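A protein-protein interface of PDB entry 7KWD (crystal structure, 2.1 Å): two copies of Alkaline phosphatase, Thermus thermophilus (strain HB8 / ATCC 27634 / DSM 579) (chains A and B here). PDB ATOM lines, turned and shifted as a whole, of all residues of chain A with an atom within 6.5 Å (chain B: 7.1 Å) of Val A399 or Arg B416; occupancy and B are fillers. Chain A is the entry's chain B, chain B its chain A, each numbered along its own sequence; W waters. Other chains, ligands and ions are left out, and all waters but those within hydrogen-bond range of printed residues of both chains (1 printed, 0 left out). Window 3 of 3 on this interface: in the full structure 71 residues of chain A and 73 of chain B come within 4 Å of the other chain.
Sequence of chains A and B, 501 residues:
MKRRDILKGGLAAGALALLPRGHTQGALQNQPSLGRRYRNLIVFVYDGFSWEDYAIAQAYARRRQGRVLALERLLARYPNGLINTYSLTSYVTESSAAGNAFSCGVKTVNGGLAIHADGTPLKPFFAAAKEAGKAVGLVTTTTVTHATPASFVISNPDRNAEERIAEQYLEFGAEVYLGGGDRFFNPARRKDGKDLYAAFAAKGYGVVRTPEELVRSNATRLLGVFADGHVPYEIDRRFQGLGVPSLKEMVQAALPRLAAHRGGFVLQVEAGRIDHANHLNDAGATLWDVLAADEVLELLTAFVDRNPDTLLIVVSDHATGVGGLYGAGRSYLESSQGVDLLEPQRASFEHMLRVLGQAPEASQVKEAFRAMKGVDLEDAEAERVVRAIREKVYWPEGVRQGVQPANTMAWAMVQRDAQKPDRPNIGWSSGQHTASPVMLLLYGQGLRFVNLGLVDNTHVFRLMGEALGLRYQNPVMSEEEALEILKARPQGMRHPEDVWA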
ATOM      1  N   GLU A 397      13.813 -26.840  23.726  1.00  0.00           N
ATOM      2  CA  GLU A 397      13.320 -27.133  22.383  1.00  0.00           C
ATOM      3  C   GLU A 397      13.284 -28.648  22.227  1.00  0.00           C
ATOM      4  O   GLU A 397      13.525 -29.396  23.182  1.00  0.00           O
ATOM      5  CB  GLU A 397      14.147 -26.450  21.291  1.00  0.00           C
ATOM      6  CG  GLU A 397      15.641 -26.658  21.390  1.00  0.00           C
ATOM      7  CD  GLU A 397      16.029 -27.996  20.839  1.00  0.00           C
ATOM      8  OE1 GLU A 397      15.899 -28.176  19.610  1.00  0.00           O
ATOM      9  OE2 GLU A 397      16.399 -28.864  21.652  1.00  0.00           O
ATOM     10  N   GLY A 398      12.917 -29.101  21.025  1.00  0.00           N
ATOM     11  CA  GLY A 398      12.538 -30.496  20.852  1.00  0.00           C
ATOM     12  C   GLY A 398      13.216 -31.206  19.696  1.00  0.00           C
ATOM     13  O   GLY A 398      12.808 -32.304  19.289  1.00  0.00           O
ATOM     14  N   VAL A 399      14.254 -30.576  19.162  1.00  0.00           N
ATOM     15  CA  VAL A 399      14.988 -31.086  18.011  1.00  0.00           C
ATOM     16  C   VAL A 399      16.386 -31.566  18.412  1.00  0.00           C
ATOM     17  O   VAL A 399      16.721 -32.740  18.242  1.00  0.00           O
ATOM     18  CB  VAL A 399      15.058 -30.021  16.898  1.00  0.00           C
ATOM     19  CG1 VAL A 399      16.089 -30.374  15.886  1.00  0.00           C
ATOM     20  CG2 VAL A 399      13.663 -29.860  16.250  1.00  0.00           C
ATOM     21  N   ARG A 400      17.222 -30.662  18.913  1.00  0.00           N
ATOM     22  CA  ARG A 400      18.462 -31.059  19.564  1.00  0.00           C
ATOM     23  C   ARG A 400      18.160 -31.979  20.733  1.00  0.00           C
ATOM     24  O   ARG A 400      18.740 -33.059  20.858  1.00  0.00           O
ATOM     25  CB  ARG A 400      19.222 -29.811  20.015  1.00  0.00           C
ATOM     26  CG  ARG A 400      20.450 -30.090  20.937  1.00  0.00           C
ATOM     27  CD  ARG A 400      21.381 -28.871  20.973  1.00  0.00           C
ATOM     28  NE  ARG A 400      22.117 -28.758  22.228  1.00  0.00           N
ATOM     29  CZ  ARG A 400      23.010 -27.805  22.480  1.00  0.00           C
ATOM     30  NH1 ARG A 400      23.264 -26.900  21.565  1.00  0.00           N
ATOM     31  NH2 ARG A 400      23.654 -27.769  23.649  1.00  0.00           N
ATOM     32  N   GLN A 401      17.190 -31.596  21.564  1.00  0.00           N
ATOM     33  CA  GLN A 401      16.661 -32.452  22.619  1.00  0.00           C
ATOM     34  C   GLN A 401      15.414 -33.145  22.074  1.00  0.00           C
ATOM     35  O   GLN A 401      14.271 -32.780  22.380  1.00  0.00           O
ATOM     36  CB  GLN A 401      16.360 -31.622  23.865  1.00  0.00           C
ATOM     37  CG  GLN A 401      17.585 -30.816  24.329  1.00  0.00           C
ATOM     38  CD  GLN A 401      18.585 -31.625  25.194  1.00  0.00           C
ATOM     39  OE1 GLN A 401      19.509 -31.044  25.737  1.00  0.00           O
ATOM     40  NE2 GLN A 401      18.392 -32.945  25.305  1.00  0.00           N
ATOM     41  N   GLY A 402      15.649 -34.177  21.271  1.00  0.00           N
ATOM     42  CA  GLY A 402      14.629 -34.856  20.503  1.00  0.00           C
ATOM     43  C   GLY A 402      13.842 -35.912  21.213  1.00  0.00           C
ATOM     44  O   GLY A 402      12.989 -36.541  20.583  1.00  0.00           O
ATOM     45  N   VAL A 403      14.063 -36.124  22.503  1.00  0.00           N
ATOM     46  CA  VAL A 403      13.344 -37.158  23.242  1.00  0.00           C
ATOM     47  C   VAL A 403      12.539 -36.465  24.328  1.00  0.00           C
ATOM     48  O   VAL A 403      13.107 -35.825  25.214  1.00  0.00           O
ATOM     49  CB  VAL A 403      14.292 -38.214  23.826  1.00  0.00           C
ATOM     50  CG1 VAL A 403      13.544 -39.160  24.728  1.00  0.00           C
ATOM     51  CG2 VAL A 403      14.991 -39.018  22.674  1.00  0.00           C
ATOM     52  N   GLN A 404      11.218 -36.581  24.252  1.00  0.00           N
ATOM     53  CA  GLN A 404      10.335 -35.732  25.040  1.00  0.00           C
ATOM     54  C   GLN A 404       9.176 -36.557  25.549  1.00  0.00           C
ATOM     55  O   GLN A 404       8.738 -37.496  24.876  1.00  0.00           O
ATOM     56  CB  GLN A 404       9.802 -34.569  24.200  1.00  0.00           C
ATOM     57  CG  GLN A 404      10.893 -33.633  23.771  1.00  0.00           C
ATOM     58  CD  GLN A 404      11.487 -32.875  24.944  1.00  0.00           C
ATOM     59  OE1 GLN A 404      10.981 -32.948  26.075  1.00  0.00           O
ATOM     60  NE2 GLN A 404      12.570 -32.132  24.682  1.00  0.00           N
ATOM     61  N   SER A 430      22.575 -33.945  23.479  1.00  0.00           N
ATOM     62  CA  SER A 430      21.403 -34.197  22.657  1.00  0.00           C
ATOM     63  C   SER A 430      20.612 -35.316  23.303  1.00  0.00           C
ATOM     64  O   SER A 430      21.034 -35.877  24.331  1.00  0.00           O
ATOM     65  CB  SER A 430      21.805 -34.606  21.238  1.00  0.00           C
ATOM     66  OG  SER A 430      22.013 -36.017  21.221  1.00  0.00           O
ATOM     67  N   GLY A 431      19.474 -35.652  22.718  1.00  0.00           N
ATOM     68  CA  GLY A 431      18.697 -36.797  23.106  1.00  0.00           C
ATOM     69  C   GLY A 431      18.932 -37.976  22.204  1.00  0.00           C
ATOM     70  O   GLY A 431      18.157 -38.947  22.252  1.00  0.00           O
ATOM     71  N   GLN A 432      19.961 -37.936  21.370  1.00  0.00           N
ATOM     72  CA  GLN A 432      20.140 -38.903  20.305  1.00  0.00           C
ATOM     73  C   GLN A 432      21.534 -39.516  20.345  1.00  0.00           C
ATOM     74  O   GLN A 432      22.399 -39.096  21.115  1.00  0.00           O
ATOM     75  CB  GLN A 432      19.893 -38.238  18.945  1.00  0.00           C
ATOM     76  CG  GLN A 432      18.439 -37.773  18.744  1.00  0.00           C
ATOM     77  CD  GLN A 432      18.201 -36.356  19.284  1.00  0.00           C
ATOM     78  OE1 GLN A 432      17.635 -36.177  20.371  1.00  0.00           O
ATOM     79  NE2 GLN A 432      18.666 -35.349  18.536  1.00  0.00           N
ATOM     80  N   TYR B 326      25.038 -35.402  16.365  1.00  0.00           N
ATOM     81  CA  TYR B 326      23.994 -36.246  16.919  1.00  0.00           C
ATOM     82  C   TYR B 326      22.995 -36.658  15.845  1.00  0.00           C
ATOM     83  O   TYR B 326      22.928 -36.074  14.767  1.00  0.00           O
ATOM     84  CB  TYR B 326      23.262 -35.547  18.087  1.00  0.00           C
ATOM     85  CG  TYR B 326      22.541 -34.267  17.705  1.00  0.00           C
ATOM     86  CD1 TYR B 326      21.318 -34.308  17.040  1.00  0.00           C
ATOM     87  CD2 TYR B 326      23.066 -33.017  18.049  1.00  0.00           C
ATOM     88  CE1 TYR B 326      20.657 -33.116  16.689  1.00  0.00           C
ATOM     89  CE2 TYR B 326      22.416 -31.851  17.711  1.00  0.00           C
ATOM     90  CZ  TYR B 326      21.210 -31.906  17.022  1.00  0.00           C
ATOM     91  OH  TYR B 326      20.586 -30.718  16.694  1.00  0.00           O
ATOM     92  N   GLY B 327      22.221 -37.687  16.187  1.00  0.00           N
ATOM     93  CA  GLY B 327      21.332 -38.306  15.218  1.00  0.00           C
ATOM     94  C   GLY B 327      20.245 -37.339  14.800  1.00  0.00           C
ATOM     95  O   GLY B 327      19.593 -36.718  15.642  1.00  0.00           O
ATOM     96  N   ALA B 328      20.043 -37.218  13.490  1.00  0.00           N
ATOM     97  CA  ALA B 328      19.133 -36.259  12.879  1.00  0.00           C
ATOM     98  C   ALA B 328      18.385 -36.904  11.717  1.00  0.00           C
ATOM     99  O   ALA B 328      18.978 -37.584  10.873  1.00  0.00           O
ATOM    100  CB  ALA B 328      19.907 -35.038  12.386  1.00  0.00           C
ATOM    101  N   VAL B 375      24.207 -18.964   8.508  1.00  0.00           N
ATOM    102  CA  VAL B 375      22.980 -19.247   9.243  1.00  0.00           C
ATOM    103  C   VAL B 375      22.047 -18.048   9.099  1.00  0.00           C
ATOM    104  O   VAL B 375      22.496 -16.897   9.164  1.00  0.00           O
ATOM    105  CB  VAL B 375      23.273 -19.520  10.740  1.00  0.00           C
ATOM    106  CG1 VAL B 375      22.017 -19.370  11.616  1.00  0.00           C
ATOM    107  CG2 VAL B 375      23.873 -20.913  10.925  1.00  0.00           C
ATOM    108  N   ASP B 376      20.749 -18.328   8.927  1.00  0.00           N
ATOM    109  CA  ASP B 376      19.707 -17.302   8.794  1.00  0.00           C
ATOM    110  C   ASP B 376      18.865 -17.352  10.061  1.00  0.00           C
ATOM    111  O   ASP B 376      17.968 -18.188  10.192  1.00  0.00           O
ATOM    112  CB  ASP B 376      18.849 -17.531   7.550  1.00  0.00           C
ATOM    113  CG  ASP B 376      19.617 -17.292   6.262  1.00  0.00           C
ATOM    114  OD1 ASP B 376      20.364 -16.281   6.185  1.00  0.00           O
ATOM    115  OD2 ASP B 376      19.486 -18.122   5.328  1.00  0.00           O
ATOM    116  N   LEU B 377      19.175 -16.464  10.998  1.00  0.00           N
ATOM    117  CA  LEU B 377      18.504 -16.443  12.284  1.00  0.00           C
ATOM    118  C   LEU B 377      17.107 -15.839  12.190  1.00  0.00           C
ATOM    119  O   LEU B 377      16.869 -14.885  11.446  1.00  0.00           O
ATOM    120  CB  LEU B 377      19.332 -15.629  13.276  1.00  0.00           C
ATOM    121  CG  LEU B 377      20.530 -16.316  13.930  1.00  0.00           C
ATOM    122  CD1 LEU B 377      21.189 -15.326  14.904  1.00  0.00           C
ATOM    123  CD2 LEU B 377      20.119 -17.582  14.648  1.00  0.00           C
ATOM    124  N   GLU B 378      16.195 -16.391  12.977  1.00  0.00           N
ATOM    125  CA  GLU B 378      14.926 -15.759  13.238  1.00  0.00           C
ATOM    126  C   GLU B 378      15.121 -14.544  14.142  1.00  0.00           C
ATOM    127  O   GLU B 378      16.097 -14.446  14.898  1.00  0.00           O
ATOM    128  CB  GLU B 378      13.970 -16.744  13.912  1.00  0.00           C
ATOM    129  CG  GLU B 378      13.506 -17.906  13.049  1.00  0.00           C
ATOM    130  CD  GLU B 378      12.722 -18.933  13.855  1.00  0.00           C
ATOM    131  OE1 GLU B 378      12.057 -18.521  14.829  1.00  0.00           O
ATOM    132  OE2 GLU B 378      12.768 -20.147  13.527  1.00  0.00           O
ATOM    133  N   GLU B 381      15.745 -15.244  17.738  1.00  0.00           N
ATOM    134  CA  GLU B 381      17.058 -15.817  18.016  1.00  0.00           C
ATOM    135  C   GLU B 381      18.099 -14.712  18.068  1.00  0.00           C
ATOM    136  O   GLU B 381      18.908 -14.654  18.998  1.00  0.00           O
ATOM    137  CB  GLU B 381      17.399 -16.875  16.960  1.00  0.00           C
ATOM    138  CG  GLU B 381      16.462 -18.111  17.004  1.00  0.00           C
ATOM    139  CD  GLU B 381      16.663 -19.040  15.827  1.00  0.00           C
ATOM    140  OE1 GLU B 381      16.970 -18.528  14.725  1.00  0.00           O
ATOM    141  OE2 GLU B 381      16.502 -20.275  16.000  1.00  0.00           O
ATOM    142  N   ALA B 412      21.222 -20.143  19.824  1.00  0.00           N
ATOM    143  CA  ALA B 412      20.504 -19.301  18.873  1.00  0.00           C
ATOM    144  C   ALA B 412      20.523 -19.897  17.471  1.00  0.00           C
ATOM    145  O   ALA B 412      19.572 -19.694  16.704  1.00  0.00           O
ATOM    146  CB  ALA B 412      21.100 -17.890  18.892  1.00  0.00           C
ATOM    147  N   MET B 413      21.574 -20.661  17.124  1.00  0.00           N
ATOM    148  CA  MET B 413      21.674 -21.274  15.805  1.00  0.00           C
ATOM    149  C   MET B 413      21.450 -22.784  15.853  1.00  0.00           C
ATOM    150  O   MET B 413      22.027 -23.530  15.061  1.00  0.00           O
ATOM    151  CB  MET B 413      23.019 -20.947  15.157  1.00  0.00           C
ATOM    152  CG  MET B 413      24.236 -21.533  15.852  1.00  0.00           C
ATOM    153  SD  MET B 413      25.736 -20.984  14.994  1.00  0.00           S
ATOM    154  CE  MET B 413      25.834 -22.132  13.642  1.00  0.00           C
ATOM    155  N   VAL B 414      20.596 -23.238  16.764  1.00  0.00           N
ATOM    156  CA  VAL B 414      20.279 -24.651  16.864  1.00  0.00           C
ATOM    157  C   VAL B 414      19.504 -25.095  15.634  1.00  0.00           C
ATOM    158  O   VAL B 414      18.776 -24.324  15.010  1.00  0.00           O
ATOM    159  CB  VAL B 414      19.494 -24.917  18.161  1.00  0.00           C
ATOM    160  CG1 VAL B 414      18.166 -24.184  18.121  1.00  0.00           C
ATOM    161  CG2 VAL B 414      19.219 -26.376  18.386  1.00  0.00           C
ATOM    162  N   GLN B 415      19.696 -26.358  15.275  1.00  0.00           N
ATOM    163  CA  GLN B 415      18.859 -27.051  14.311  1.00  0.00           C
ATOM    164  C   GLN B 415      17.386 -26.851  14.611  1.00  0.00           C
ATOM    165  O   GLN B 415      16.937 -27.012  15.753  1.00  0.00           O
ATOM    166  CB  GLN B 415      19.188 -28.550  14.348  1.00  0.00           C
ATOM    167  CG  GLN B 415      18.555 -29.412  13.234  1.00  0.00           C
ATOM    168  CD  GLN B 415      18.556 -30.906  13.562  1.00  0.00           C
ATOM    169  OE1 GLN B 415      19.336 -31.380  14.399  1.00  0.00           O
ATOM    170  NE2 GLN B 415      17.677 -31.654  12.910  1.00  0.00           N
ATOM    171  N   ARG B 416      16.633 -26.510  13.573  1.00  0.00           N
ATOM    172  CA  ARG B 416      15.180 -26.369  13.665  1.00  0.00           C
ATOM    173  C   ARG B 416      14.430 -27.390  12.820  1.00  0.00           C
ATOM    174  O   ARG B 416      13.331 -27.807  13.190  1.00  0.00           O
ATOM    175  CB  ARG B 416      14.750 -24.961  13.212  1.00  0.00           C
ATOM    176  CG  ARG B 416      15.320 -23.821  14.005  1.00  0.00           C
ATOM    177  CD  ARG B 416      15.031 -22.508  13.298  1.00  0.00           C
ATOM    178  NE  ARG B 416      15.744 -22.451  12.022  1.00  0.00           N
ATOM    179  CZ  ARG B 416      15.560 -21.527  11.078  1.00  0.00           C
ATOM    180  NH1 ARG B 416      14.667 -20.551  11.239  1.00  0.00           N
ATOM    181  NH2 ARG B 416      16.281 -21.581   9.967  1.00  0.00           N
ATOM    182  N   ASP B 417      14.999 -27.812  11.700  1.00  0.00           N
ATOM    183  CA  ASP B 417      14.327 -28.713  10.770  1.00  0.00           C
ATOM    184  C   ASP B 417      14.648 -30.144  11.183  1.00  0.00           C
ATOM    185  O   ASP B 417      15.731 -30.663  10.893  1.00  0.00           O
ATOM    186  CB  ASP B 417      14.794 -28.404   9.351  1.00  0.00           C
ATOM    187  CG  ASP B 417      14.047 -29.175   8.297  1.00  0.00           C
ATOM    188  OD1 ASP B 417      13.472 -30.254   8.587  1.00  0.00           O
ATOM    189  OD2 ASP B 417      14.062 -28.696   7.152  1.00  0.00           O
ATOM    190  N   ALA B 418      13.685 -30.794  11.834  1.00  0.00           N
ATOM    191  CA  ALA B 418      13.918 -32.130  12.352  1.00  0.00           C
ATOM    192  C   ALA B 418      14.016 -33.186  11.257  1.00  0.00           C
ATOM    193  O   ALA B 418      14.471 -34.287  11.537  1.00  0.00           O
ATOM    194  CB  ALA B 418      12.797 -32.511  13.314  1.00  0.00           C
ATOM    195  N   GLN B 419      13.587 -32.878  10.026  1.00  0.00           N
ATOM    196  CA  GLN B 419      13.628 -33.866   8.956  1.00  0.00           C
ATOM    197  C   GLN B 419      15.007 -33.913   8.328  1.00  0.00           C
ATOM    198  O   GLN B 419      15.465 -34.975   7.895  1.00  0.00           O
ATOM    199  CB  GLN B 419      12.595 -33.554   7.858  1.00  0.00           C
ATOM    200  CG  GLN B 419      11.139 -33.582   8.320  1.00  0.00           C
ATOM    201  CD  GLN B 419      10.809 -34.803   9.177  1.00  0.00           C
ATOM    202  OE1 GLN B 419      10.131 -34.696  10.208  1.00  0.00           O
ATOM    203  NE2 GLN B 419      11.297 -35.973   8.752  1.00  0.00           N
ATOM    204  N   LYS B 420      15.651 -32.756   8.245  1.00  0.00           N
ATOM    205  CA  LYS B 420      16.969 -32.591   7.644  1.00  0.00           C
ATOM    206  C   LYS B 420      17.608 -31.345   8.245  1.00  0.00           C
ATOM    207  O   LYS B 420      17.030 -30.260   8.153  1.00  0.00           O
ATOM    208  CB  LYS B 420      16.856 -32.482   6.130  1.00  0.00           C
ATOM    209  CG  LYS B 420      18.143 -32.776   5.395  1.00  0.00           C
ATOM    210  CD  LYS B 420      17.873 -32.904   3.896  1.00  0.00           C
ATOM    211  CE  LYS B 420      19.137 -33.150   3.080  1.00  0.00           C
ATOM    212  NZ  LYS B 420      18.900 -32.993   1.610  1.00  0.00           N
ATOM    213  N   PRO B 421      18.758 -31.465   8.914  1.00  0.00           N
ATOM    214  CA  PRO B 421      19.351 -30.287   9.563  1.00  0.00           C
ATOM    215  C   PRO B 421      19.458 -29.103   8.616  1.00  0.00           C
ATOM    216  O   PRO B 421      19.998 -29.209   7.507  1.00  0.00           O
ATOM    217  CB  PRO B 421      20.734 -30.786  10.016  1.00  0.00           C
ATOM    218  CG  PRO B 421      20.488 -32.206  10.387  1.00  0.00           C
ATOM    219  CD  PRO B 421      19.395 -32.719   9.388  1.00  0.00           C
ATOM    220  N   ASP B 422      18.896 -27.973   9.055  1.00  0.00           N
ATOM    221  CA  ASP B 422      19.122 -26.689   8.409  1.00  0.00           C
ATOM    222  C   ASP B 422      20.314 -25.964   8.996  1.00  0.00           C
ATOM    223  O   ASP B 422      20.875 -25.075   8.346  1.00  0.00           O
ATOM    224  CB  ASP B 422      17.882 -25.798   8.524  1.00  0.00           C
ATOM    225  CG  ASP B 422      17.424 -25.581   9.970  1.00  0.00           C
ATOM    226  OD1 ASP B 422      17.498 -26.523  10.805  1.00  0.00           O
ATOM    227  OD2 ASP B 422      16.960 -24.450  10.253  1.00  0.00           O
ATOM    228  N   ARG B 423      20.688 -26.312  10.218  1.00  0.00           N
ATOM    229  CA  ARG B 423      21.890 -25.838  10.886  1.00  0.00           C
ATOM    230  C   ARG B 423      22.536 -27.039  11.545  1.00  0.00           C
ATOM    231  O   ARG B 423      21.882 -28.077  11.740  1.00  0.00           O
ATOM    232  CB  ARG B 423      21.553 -24.741  11.900  1.00  0.00           C
ATOM    233  CG  ARG B 423      20.571 -23.714  11.346  1.00  0.00           C
ATOM    234  CD  ARG B 423      19.862 -23.095  12.503  1.00  0.00           C
ATOM    235  NE  ARG B 423      19.202 -21.852  12.150  1.00  0.00           N
ATOM    236  CZ  ARG B 423      18.473 -21.155  13.010  1.00  0.00           C
ATOM    237  NH1 ARG B 423      18.313 -21.607  14.246  1.00  0.00           N
ATOM    238  NH2 ARG B 423      17.901 -20.021  12.637  1.00  0.00           N
ATOM    239  N   ASN B 425      23.594 -30.188  13.257  1.00  0.00           N
ATOM    240  CA  ASN B 425      23.160 -31.088  14.315  1.00  0.00           C
ATOM    241  C   ASN B 425      24.331 -31.517  15.213  1.00  0.00           C
ATOM    242  O   ASN B 425      24.604 -32.706  15.411  1.00  0.00           O
ATOM    243  CB  ASN B 425      22.457 -32.301  13.718  1.00  0.00           C
ATOM    244  CG  ASN B 425      23.254 -32.965  12.622  1.00  0.00           C
ATOM    245  OD1 ASN B 425      23.648 -32.330  11.646  1.00  0.00           O
ATOM    246  ND2 ASN B 425      23.499 -34.262  12.780  1.00  0.00           N
HETATM  247  O   HOH W   1      15.189 -26.517  17.658  1.00  0.00           O
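Among the printed residues, merely in contact across the chains: Glu A397 with Val B414, Val A399 with Gln B415, Val A399 with Arg B416, Arg A400 with Tyr B326, Arg A400 with Val B414, Ser A430 with Tyr B326 and Gln A432 with Tyr B326.
Water W1 bridges the backbone carbonyl oxygen of Gln B415 (2.6 Å) and the side-chain carboxylate of Glu A397 (2.7 Å).
NE2 of Gln B415 sits at hydrogen-bond distance from O of Asp B417, 3.0 Å away. The side-chain carboxylate (OE1) of Glu A397 lies within hydrogen-bond range of the backbone NH (N) of Arg A400 (2.9 Å). The side-chain amide nitrogen of Gln A432 lies within hydrogen-bond range of the backbone carbonyl oxygen of Val A399, 3.3 Å away. The backbone NH (N) of Gly A431 sits at hydrogen-bond distance from the backbone carbonyl oxygen (O) of Arg A400, 3.3 Å away. O of Arg A400 is in hydrogen-bond range of NE2 of Gln A432, 3.3 Å away. N of Gln A432 is in hydrogen-bond range of OG of Ser A430, at 2.8 Å.
Of chain B, only Gln B415 and Arg B416 come within 4 Å of Val A399. Arg B416 touches just one residue of chain A: Val A399 (3.7 Å). Of the printed residues of chain B, Arg A400 touches Tyr B326 and Val B414. Of the printed residues of chain A, Gly B327 touches Gln A432 (3.3 Å). Printed residues of chain A within 4 Å of Gln B415: Val A399. The nearest residue of chain B that does not touch Val A399 is Ala B418 (4.05 Å). The nearest residue of chain A that does not touch Arg B416 is Glu A397 (6.3 Å). The nearest printed residue of chain A that does not touch Gly B327 is Ser A430 (5.3 Å).
The backbone carbonyl oxygen of Gly B327 sits at hydrogen-bond distance from the side-chain amide nitrogen of Gln A432, 3.3 Å away.
Of the 21 printed residues of chain B, 5 touch a printed residue of chain A. Of the 11 printed residues of chain A, 5 touch a printed residue of chain B. Along chain A the printed residues that touch a printed residue of chain B span positions 397 to 432.
No position is printed for both chains. Of the 8 pairs that touch across the chains among the printed residues, none has its exchanged pair printed and touching as well.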
